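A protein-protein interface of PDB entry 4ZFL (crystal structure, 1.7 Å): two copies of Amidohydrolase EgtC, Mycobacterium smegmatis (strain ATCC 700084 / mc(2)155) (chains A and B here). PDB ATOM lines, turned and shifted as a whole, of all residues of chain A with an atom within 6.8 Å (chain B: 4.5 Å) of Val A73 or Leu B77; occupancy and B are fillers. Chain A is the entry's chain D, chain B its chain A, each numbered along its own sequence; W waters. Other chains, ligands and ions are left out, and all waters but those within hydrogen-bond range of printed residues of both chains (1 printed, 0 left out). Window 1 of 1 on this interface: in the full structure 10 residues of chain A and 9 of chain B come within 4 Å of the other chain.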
ATOM      1  N   LEU A  13     -18.827 -34.248  19.671  1.00  0.00           N
ATOM      2  CA  LEU A  13     -20.040 -33.474  19.453  1.00  0.00           C
ATOM      3  C   LEU A  13     -20.150 -33.084  17.974  1.00  0.00           C
ATOM      4  O   LEU A  13     -21.236 -33.079  17.396  1.00  0.00           O
ATOM      5  CB  LEU A  13     -20.064 -32.226  20.324  1.00  0.00           C
ATOM      6  CG  LEU A  13     -20.157 -32.383  21.855  1.00  0.00           C
ATOM      7  CD1 LEU A  13     -20.468 -31.076  22.529  1.00  0.00           C
ATOM      8  CD2 LEU A  13     -21.117 -33.441  22.291  1.00  0.00           C
ATOM      9  N   ALA A  14     -19.016 -32.759  17.363  1.00  0.00           N
ATOM     10  CA  ALA A  14     -19.028 -32.397  15.949  1.00  0.00           C
ATOM     11  C   ALA A  14     -19.484 -33.577  15.106  1.00  0.00           C
ATOM     12  O   ALA A  14     -20.300 -33.405  14.198  1.00  0.00           O
ATOM     13  CB  ALA A  14     -17.646 -31.921  15.496  1.00  0.00           C
ATOM     14  N   TRP A  58     -23.515 -26.810  26.837  1.00  0.00           N
ATOM     15  CA  TRP A  58     -23.264 -25.598  26.077  1.00  0.00           C
ATOM     16  C   TRP A  58     -24.591 -25.182  25.457  1.00  0.00           C
ATOM     17  O   TRP A  58     -25.195 -25.967  24.723  1.00  0.00           O
ATOM     18  CB  TRP A  58     -22.179 -25.887  25.018  1.00  0.00           C
ATOM     19  CG  TRP A  58     -21.611 -24.732  24.260  1.00  0.00           C
ATOM     20  CD1 TRP A  58     -22.159 -23.496  24.057  1.00  0.00           C
ATOM     21  CD2 TRP A  58     -20.349 -24.728  23.591  1.00  0.00           C
ATOM     22  NE1 TRP A  58     -21.304 -22.726  23.291  1.00  0.00           N
ATOM     23  CE2 TRP A  58     -20.186 -23.459  23.004  1.00  0.00           C
ATOM     24  CE3 TRP A  58     -19.334 -25.673  23.445  1.00  0.00           C
ATOM     25  CZ2 TRP A  58     -19.057 -23.118  22.253  1.00  0.00           C
ATOM     26  CZ3 TRP A  58     -18.212 -25.334  22.710  1.00  0.00           C
ATOM     27  CH2 TRP A  58     -18.077 -24.061  22.144  1.00  0.00           C
ATOM     28  N   ALA A  68     -19.330 -19.914  15.548  1.00  0.00           N
ATOM     29  CA  ALA A  68     -17.961 -20.226  15.130  1.00  0.00           C
ATOM     30  C   ALA A  68     -17.200 -20.930  16.238  1.00  0.00           C
ATOM     31  O   ALA A  68     -16.324 -21.753  15.976  1.00  0.00           O
ATOM     32  CB  ALA A  68     -17.251 -18.969  14.732  1.00  0.00           C
ATOM     33  N   SER A  69     -17.530 -20.581  17.479  1.00  0.00           N
ATOM     34  CA  SER A  69     -16.886 -21.209  18.632  1.00  0.00           C
ATOM     35  C   SER A  69     -17.224 -22.687  18.688  1.00  0.00           C
ATOM     36  O   SER A  69     -16.352 -23.520  18.854  1.00  0.00           O
ATOM     37  CB  SER A  69     -17.322 -20.515  19.934  1.00  0.00           C
ATOM     38  OG  SER A  69     -16.795 -19.193  19.955  1.00  0.00           O
ATOM     39  N   PHE A  70     -18.498 -23.010  18.542  1.00  0.00           N
ATOM     40  CA  PHE A  70     -18.898 -24.402  18.608  1.00  0.00           C
ATOM     41  C   PHE A  70     -18.299 -25.182  17.428  1.00  0.00           C
ATOM     42  O   PHE A  70     -17.828 -26.315  17.596  1.00  0.00           O
ATOM     43  CB  PHE A  70     -20.417 -24.525  18.629  1.00  0.00           C
ATOM     44  CG  PHE A  70     -20.896 -25.924  18.912  1.00  0.00           C
ATOM     45  CD1 PHE A  70     -20.663 -26.521  20.153  1.00  0.00           C
ATOM     46  CD2 PHE A  70     -21.567 -26.645  17.939  1.00  0.00           C
ATOM     47  CE1 PHE A  70     -21.129 -27.808  20.426  1.00  0.00           C
ATOM     48  CE2 PHE A  70     -22.012 -27.930  18.200  1.00  0.00           C
ATOM     49  CZ  PHE A  70     -21.793 -28.509  19.444  1.00  0.00           C
ATOM     50  N   ALA A  71     -18.287 -24.584  16.249  1.00  0.00           N
ATOM     51  CA  ALA A  71     -17.702 -25.257  15.092  1.00  0.00           C
ATOM     52  C   ALA A  71     -16.226 -25.575  15.342  1.00  0.00           C
ATOM     53  O   ALA A  71     -15.715 -26.610  14.921  1.00  0.00           O
ATOM     54  CB  ALA A  71     -17.844 -24.400  13.852  1.00  0.00           C
ATOM     55  N   SER A  72     -15.538 -24.681  16.042  1.00  0.00           N
ATOM     56  CA  SER A  72     -14.118 -24.850  16.315  1.00  0.00           C
ATOM     57  C   SER A  72     -13.854 -25.876  17.416  1.00  0.00           C
ATOM     58  O   SER A  72     -12.929 -26.669  17.324  1.00  0.00           O
ATOM     59  CB  SER A  72     -13.509 -23.503  16.716  1.00  0.00           C
ATOM     60  OG  SER A  72     -12.132 -23.620  17.012  1.00  0.00           O
ATOM     61  N   VAL A  73     -14.668 -25.846  18.466  1.00  0.00           N
ATOM     62  CA  VAL A  73     -14.394 -26.625  19.674  1.00  0.00           C
ATOM     63  C   VAL A  73     -15.067 -27.991  19.683  1.00  0.00           C
ATOM     64  O   VAL A  73     -14.560 -28.919  20.306  1.00  0.00           O
ATOM     65  CB  VAL A  73     -14.844 -25.826  20.929  1.00  0.00           C
ATOM     66  CG1 VAL A  73     -14.672 -26.645  22.205  1.00  0.00           C
ATOM     67  CG2 VAL A  73     -14.035 -24.528  21.028  1.00  0.00           C
ATOM     68  N   ALA A  74     -16.215 -28.106  19.024  1.00  0.00           N
ATOM     69  CA  ALA A  74     -16.991 -29.349  19.076  1.00  0.00           C
ATOM     70  C   ALA A  74     -16.206 -30.621  18.705  1.00  0.00           C
ATOM     71  O   ALA A  74     -16.457 -31.680  19.276  1.00  0.00           O
ATOM     72  CB  ALA A  74     -18.225 -29.239  18.191  1.00  0.00           C
ATOM     73  N   PRO A  75     -15.271 -30.544  17.748  1.00  0.00           N
ATOM     74  CA  PRO A  75     -14.501 -31.768  17.434  1.00  0.00           C
ATOM     75  C   PRO A  75     -13.623 -32.280  18.593  1.00  0.00           C
ATOM     76  O   PRO A  75     -13.215 -33.476  18.630  1.00  0.00           O
ATOM     77  CB  PRO A  75     -13.633 -31.327  16.255  1.00  0.00           C
ATOM     78  CG  PRO A  75     -14.363 -30.214  15.626  1.00  0.00           C
ATOM     79  CD  PRO A  75     -15.004 -29.468  16.780  1.00  0.00           C
ATOM     80  N   ALA A  76     -13.356 -31.398  19.554  1.00  0.00           N
ATOM     81  CA  ALA A  76     -12.500 -31.727  20.695  1.00  0.00           C
ATOM     82  C   ALA A  76     -13.285 -32.173  21.921  1.00  0.00           C
ATOM     83  O   ALA A  76     -12.685 -32.512  22.945  1.00  0.00           O
ATOM     84  CB  ALA A  76     -11.622 -30.522  21.065  1.00  0.00           C
ATOM     85  N   LEU A  77     -14.615 -32.188  21.823  1.00  0.00           N
ATOM     86  CA  LEU A  77     -15.480 -32.621  22.917  1.00  0.00           C
ATOM     87  C   LEU A  77     -16.050 -33.976  22.586  1.00  0.00           C
ATOM     88  O   LEU A  77     -16.897 -34.090  21.699  1.00  0.00           O
ATOM     89  CB  LEU A  77     -16.634 -31.630  23.161  1.00  0.00           C
ATOM     90  CG  LEU A  77     -16.193 -30.304  23.785  1.00  0.00           C
ATOM     91  CD1 LEU A  77     -17.303 -29.257  23.702  1.00  0.00           C
ATOM     92  CD2 LEU A  77     -15.759 -30.531  25.223  1.00  0.00           C
ATOM     93  N   ARG B  11      -3.477 -29.225  30.927  1.00  0.00           N
ATOM     94  CA  ARG B  11      -4.243 -28.589  31.987  1.00  0.00           C
ATOM     95  C   ARG B  11      -5.595 -28.215  31.375  1.00  0.00           C
ATOM     96  O   ARG B  11      -5.683 -27.935  30.171  1.00  0.00           O
ATOM     97  CB  ARG B  11      -3.548 -27.349  32.563  1.00  0.00           C
ATOM     98  CG  ARG B  11      -2.372 -27.658  33.492  1.00  0.00           C
ATOM     99  CD  ARG B  11      -1.750 -26.381  34.036  1.00  0.00           C
ATOM    100  NE  ARG B  11      -2.613 -25.680  34.991  1.00  0.00           N
ATOM    101  CZ  ARG B  11      -2.288 -24.550  35.609  1.00  0.00           C
ATOM    102  NH1 ARG B  11      -1.110 -23.988  35.379  1.00  0.00           N
ATOM    103  NH2 ARG B  11      -3.134 -23.984  36.470  1.00  0.00           N
ATOM    104  N   SER B  12      -6.661 -28.275  32.162  1.00  0.00           N
ATOM    105  CA  SER B  12      -7.971 -27.896  31.637  1.00  0.00           C
ATOM    106  C   SER B  12      -8.087 -26.383  31.523  1.00  0.00           C
ATOM    107  O   SER B  12      -7.396 -25.626  32.193  1.00  0.00           O
ATOM    108  CB  SER B  12      -9.091 -28.427  32.521  1.00  0.00           C
ATOM    109  OG  SER B  12      -9.261 -27.590  33.647  1.00  0.00           O
ATOM    110  N   LEU B  13      -8.961 -25.927  30.642  1.00  0.00           N
ATOM    111  CA  LEU B  13      -9.224 -24.505  30.531  1.00  0.00           C
ATOM    112  C   LEU B  13      -9.746 -23.966  31.875  1.00  0.00           C
ATOM    113  O   LEU B  13      -9.380 -22.866  32.304  1.00  0.00           O
ATOM    114  CB  LEU B  13     -10.255 -24.241  29.432  1.00  0.00           C
ATOM    115  CG  LEU B  13      -9.864 -24.554  27.980  1.00  0.00           C
ATOM    116  CD1 LEU B  13     -10.895 -24.049  26.993  1.00  0.00           C
ATOM    117  CD2 LEU B  13      -8.477 -24.066  27.609  1.00  0.00           C
ATOM    118  N   PHE B  48      -6.762 -23.046  22.348  1.00  0.00           N
ATOM    119  CA  PHE B  48      -5.910 -24.140  22.771  1.00  0.00           C
ATOM    120  C   PHE B  48      -5.553 -24.998  21.575  1.00  0.00           C
ATOM    121  O   PHE B  48      -6.174 -24.904  20.502  1.00  0.00           O
ATOM    122  CB  PHE B  48      -6.601 -24.967  23.864  1.00  0.00           C
ATOM    123  CG  PHE B  48      -7.844 -25.669  23.388  1.00  0.00           C
ATOM    124  CD1 PHE B  48      -9.039 -24.994  23.323  1.00  0.00           C
ATOM    125  CD2 PHE B  48      -7.802 -26.981  22.981  1.00  0.00           C
ATOM    126  CE1 PHE B  48     -10.196 -25.625  22.874  1.00  0.00           C
ATOM    127  CE2 PHE B  48      -8.957 -27.627  22.534  1.00  0.00           C
ATOM    128  CZ  PHE B  48     -10.154 -26.930  22.477  1.00  0.00           C
ATOM    129  N   ARG B  57     -10.639 -22.425  19.182  1.00  0.00           N
ATOM    130  CA  ARG B  57     -10.969 -21.226  19.906  1.00  0.00           C
ATOM    131  C   ARG B  57     -12.425 -21.112  20.235  1.00  0.00           C
ATOM    132  O   ARG B  57     -13.295 -21.333  19.391  1.00  0.00           O
ATOM    133  CB  ARG B  57     -10.573 -19.966  19.107  1.00  0.00           C
ATOM    134  CG  ARG B  57      -9.073 -19.756  18.939  1.00  0.00           C
ATOM    135  CD  ARG B  57      -8.822 -18.465  18.182  1.00  0.00           C
ATOM    136  NE  ARG B  57      -9.318 -18.550  16.809  1.00  0.00           N
ATOM    137  CZ  ARG B  57      -9.449 -17.500  15.999  1.00  0.00           C
ATOM    138  NH1 ARG B  57      -9.139 -16.291  16.431  1.00  0.00           N
ATOM    139  NH2 ARG B  57      -9.896 -17.661  14.759  1.00  0.00           N
ATOM    140  N   TRP B  58     -12.664 -20.713  21.475  1.00  0.00           N
ATOM    141  CA  TRP B  58     -13.988 -20.333  21.965  1.00  0.00           C
ATOM    142  C   TRP B  58     -13.900 -18.854  22.282  1.00  0.00           C
ATOM    143  O   TRP B  58     -13.088 -18.457  23.099  1.00  0.00           O
ATOM    144  CB  TRP B  58     -14.348 -21.163  23.208  1.00  0.00           C
ATOM    145  CG  TRP B  58     -15.730 -21.053  23.712  1.00  0.00           C
ATOM    146  CD1 TRP B  58     -16.632 -20.053  23.487  1.00  0.00           C
ATOM    147  CD2 TRP B  58     -16.369 -21.999  24.553  1.00  0.00           C
ATOM    148  NE1 TRP B  58     -17.810 -20.322  24.164  1.00  0.00           N
ATOM    149  CE2 TRP B  58     -17.670 -21.519  24.822  1.00  0.00           C
ATOM    150  CE3 TRP B  58     -15.963 -23.220  25.111  1.00  0.00           C
ATOM    151  CZ2 TRP B  58     -18.572 -22.216  25.637  1.00  0.00           C
ATOM    152  CZ3 TRP B  58     -16.868 -23.922  25.911  1.00  0.00           C
ATOM    153  CH2 TRP B  58     -18.152 -23.413  26.168  1.00  0.00           C
ATOM    154  N   VAL B  73     -18.536 -26.237  30.620  1.00  0.00           N
ATOM    155  CA  VAL B  73     -17.784 -27.065  29.681  1.00  0.00           C
ATOM    156  C   VAL B  73     -16.273 -26.987  29.859  1.00  0.00           C
ATOM    157  O   VAL B  73     -15.562 -27.943  29.528  1.00  0.00           O
ATOM    158  CB  VAL B  73     -18.158 -26.688  28.229  1.00  0.00           C
ATOM    159  CG1 VAL B  73     -17.337 -27.484  27.241  1.00  0.00           C
ATOM    160  CG2 VAL B  73     -19.648 -26.958  27.987  1.00  0.00           C
ATOM    161  N   ALA B  74     -15.755 -25.871  30.347  1.00  0.00           N
ATOM    162  CA  ALA B  74     -14.306 -25.681  30.390  1.00  0.00           C
ATOM    163  C   ALA B  74     -13.525 -26.778  31.106  1.00  0.00           C
ATOM    164  O   ALA B  74     -12.410 -27.072  30.699  1.00  0.00           O
ATOM    165  CB  ALA B  74     -13.959 -24.317  31.010  1.00  0.00           C
ATOM    166  N   PRO B  75     -14.075 -27.373  32.172  1.00  0.00           N
ATOM    167  CA  PRO B  75     -13.276 -28.431  32.821  1.00  0.00           C
ATOM    168  C   PRO B  75     -13.008 -29.658  31.940  1.00  0.00           C
ATOM    169  O   PRO B  75     -12.128 -30.476  32.241  1.00  0.00           O
ATOM    170  CB  PRO B  75     -14.137 -28.826  34.026  1.00  0.00           C
ATOM    171  CG  PRO B  75     -14.975 -27.628  34.296  1.00  0.00           C
ATOM    172  CD  PRO B  75     -15.290 -27.058  32.936  1.00  0.00           C
ATOM    173  N   ALA B  76     -13.771 -29.805  30.865  1.00  0.00           N
ATOM    174  CA  ALA B  76     -13.646 -30.970  29.999  1.00  0.00           C
ATOM    175  C   ALA B  76     -12.718 -30.715  28.812  1.00  0.00           C
ATOM    176  O   ALA B  76     -12.551 -31.591  27.974  1.00  0.00           O
ATOM    177  CB  ALA B  76     -15.032 -31.393  29.497  1.00  0.00           C
ATOM    178  N   LEU B  77     -12.162 -29.507  28.725  1.00  0.00           N
ATOM    179  CA  LEU B  77     -11.266 -29.126  27.641  1.00  0.00           C
ATOM    180  C   LEU B  77      -9.848 -28.988  28.178  1.00  0.00           C
ATOM    181  O   LEU B  77      -9.568 -28.050  28.922  1.00  0.00           O
ATOM    182  CB  LEU B  77     -11.722 -27.822  26.994  1.00  0.00           C
ATOM    183  CG  LEU B  77     -12.995 -27.926  26.147  1.00  0.00           C
ATOM    184  CD1 LEU B  77     -13.527 -26.548  25.833  1.00  0.00           C
ATOM    185  CD2 LEU B  77     -12.711 -28.678  24.879  1.00  0.00           C
ATOM    186  N   ARG B  78      -8.984 -29.931  27.814  1.00  0.00           N
ATOM    187  CA  ARG B  78      -7.601 -29.981  28.311  1.00  0.00           C
ATOM    188  C   ARG B  78      -6.607 -29.827  27.170  1.00  0.00           C
ATOM    189  O   ARG B  78      -6.854 -30.297  26.056  1.00  0.00           O
ATOM    190  CB  ARG B  78      -7.320 -31.302  29.040  1.00  0.00           C
ATOM    191  CG  ARG B  78      -7.921 -31.438  30.431  1.00  0.00           C
ATOM    192  CD  ARG B  78      -7.532 -32.792  31.061  1.00  0.00           C
ATOM    193  NE  ARG B  78      -7.985 -32.890  32.449  1.00  0.00           N
ATOM    194  N   SER B  79      -5.494 -29.154  27.431  1.00  0.00           N
ATOM    195  CA  SER B  79      -4.506 -28.917  26.387  1.00  0.00           C
ATOM    196  C   SER B  79      -3.118 -28.686  26.966  1.00  0.00           C
ATOM    197  O   SER B  79      -2.977 -28.223  28.091  1.00  0.00           O
ATOM    198  CB  SER B  79      -4.914 -27.708  25.541  1.00  0.00           C
ATOM    199  OG  SER B  79      -3.953 -27.438  24.552  1.00  0.00           O
HETATM  200  O   HOH W   1     -13.561 -20.156  16.931  1.00  0.00           O
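OG of Ser A72 is in hydrogen-bond range of N of Arg B57.
The backbone NH of Leu B13 is in hydrogen-bond range of the backbone carbonyl oxygen of Leu B77 (2.8 Å). The backbone carbonyl oxygen of Leu A77 lies within hydrogen-bond range of the backbone NH of Leu A13 (2.8 Å).
Trp A58 touches Trp B58. CA of Ser A69 touches O of Arg B57, 3.7 Å away. Trp B58 touches Ser A69 (CA to OG, 3.6 Å). Val A73 touches Arg B57 (CG2 to O, 3.7 Å). Leu B77 touches Val A73. Val B73 touches Leu A77 (CG1 to CD1, 3.96 Å). CD2 of Leu A77 touches CD2 of Leu B77, 3.6 Å away.
Of chain B, only Arg B57 (3.7 Å) and Leu B77 (3.8 Å) come within 4 Å of Val A73. Leu B77 touches two residues of chain A. Printed residues of chain B within 4 Å of Trp A58: Trp B58 (3.3 Å). Of the printed residues of chain B, Ser A69 touches Arg B57 (3.7 Å) and Trp B58 (3.6 Å). Of the printed residues of chain A, Trp B58 touches Trp A58 and Ser A69. Of the printed residues of chain A, Arg B57 touches Ser A69 (3.7 Å), Ser A72 (2.9 Å) and Val A73 (3.7 Å). Of the printed residues of chain B, Ser A72 touches Arg B57. The nearest residue of chain B that does not touch Val A73 is Trp B58 (4.02 Å). The nearest printed residue of chain A that does not touch Val B73 is Trp A58 (4.04 Å).
Of the 13 printed residues of chain A, 5 touch a printed residue of chain B. Printed residues of chain A that touch a printed residue of chain B: Trp A58, Ser A69, Ser A72, Val A73 and Leu A77.
Trp A58 touches its own counterpart, Trp B58. Val A73 touches Leu B77, and with the chains exchanged Leu A77 touches Val B73. Leu B77 touches its own counterpart, Leu A77. 7 positions are printed for both chains. Of the 8 pairs that touch across the chains among the printed residues, 4 have their exchanged pair printed and touching as well.
Water W1 lies within hydrogen-bond range of the backbone carbonyl oxygen (O) of Arg B57 (2.7 Å) and the backbone carbonyl oxygen (O) of Ala A68 (3.3 Å).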
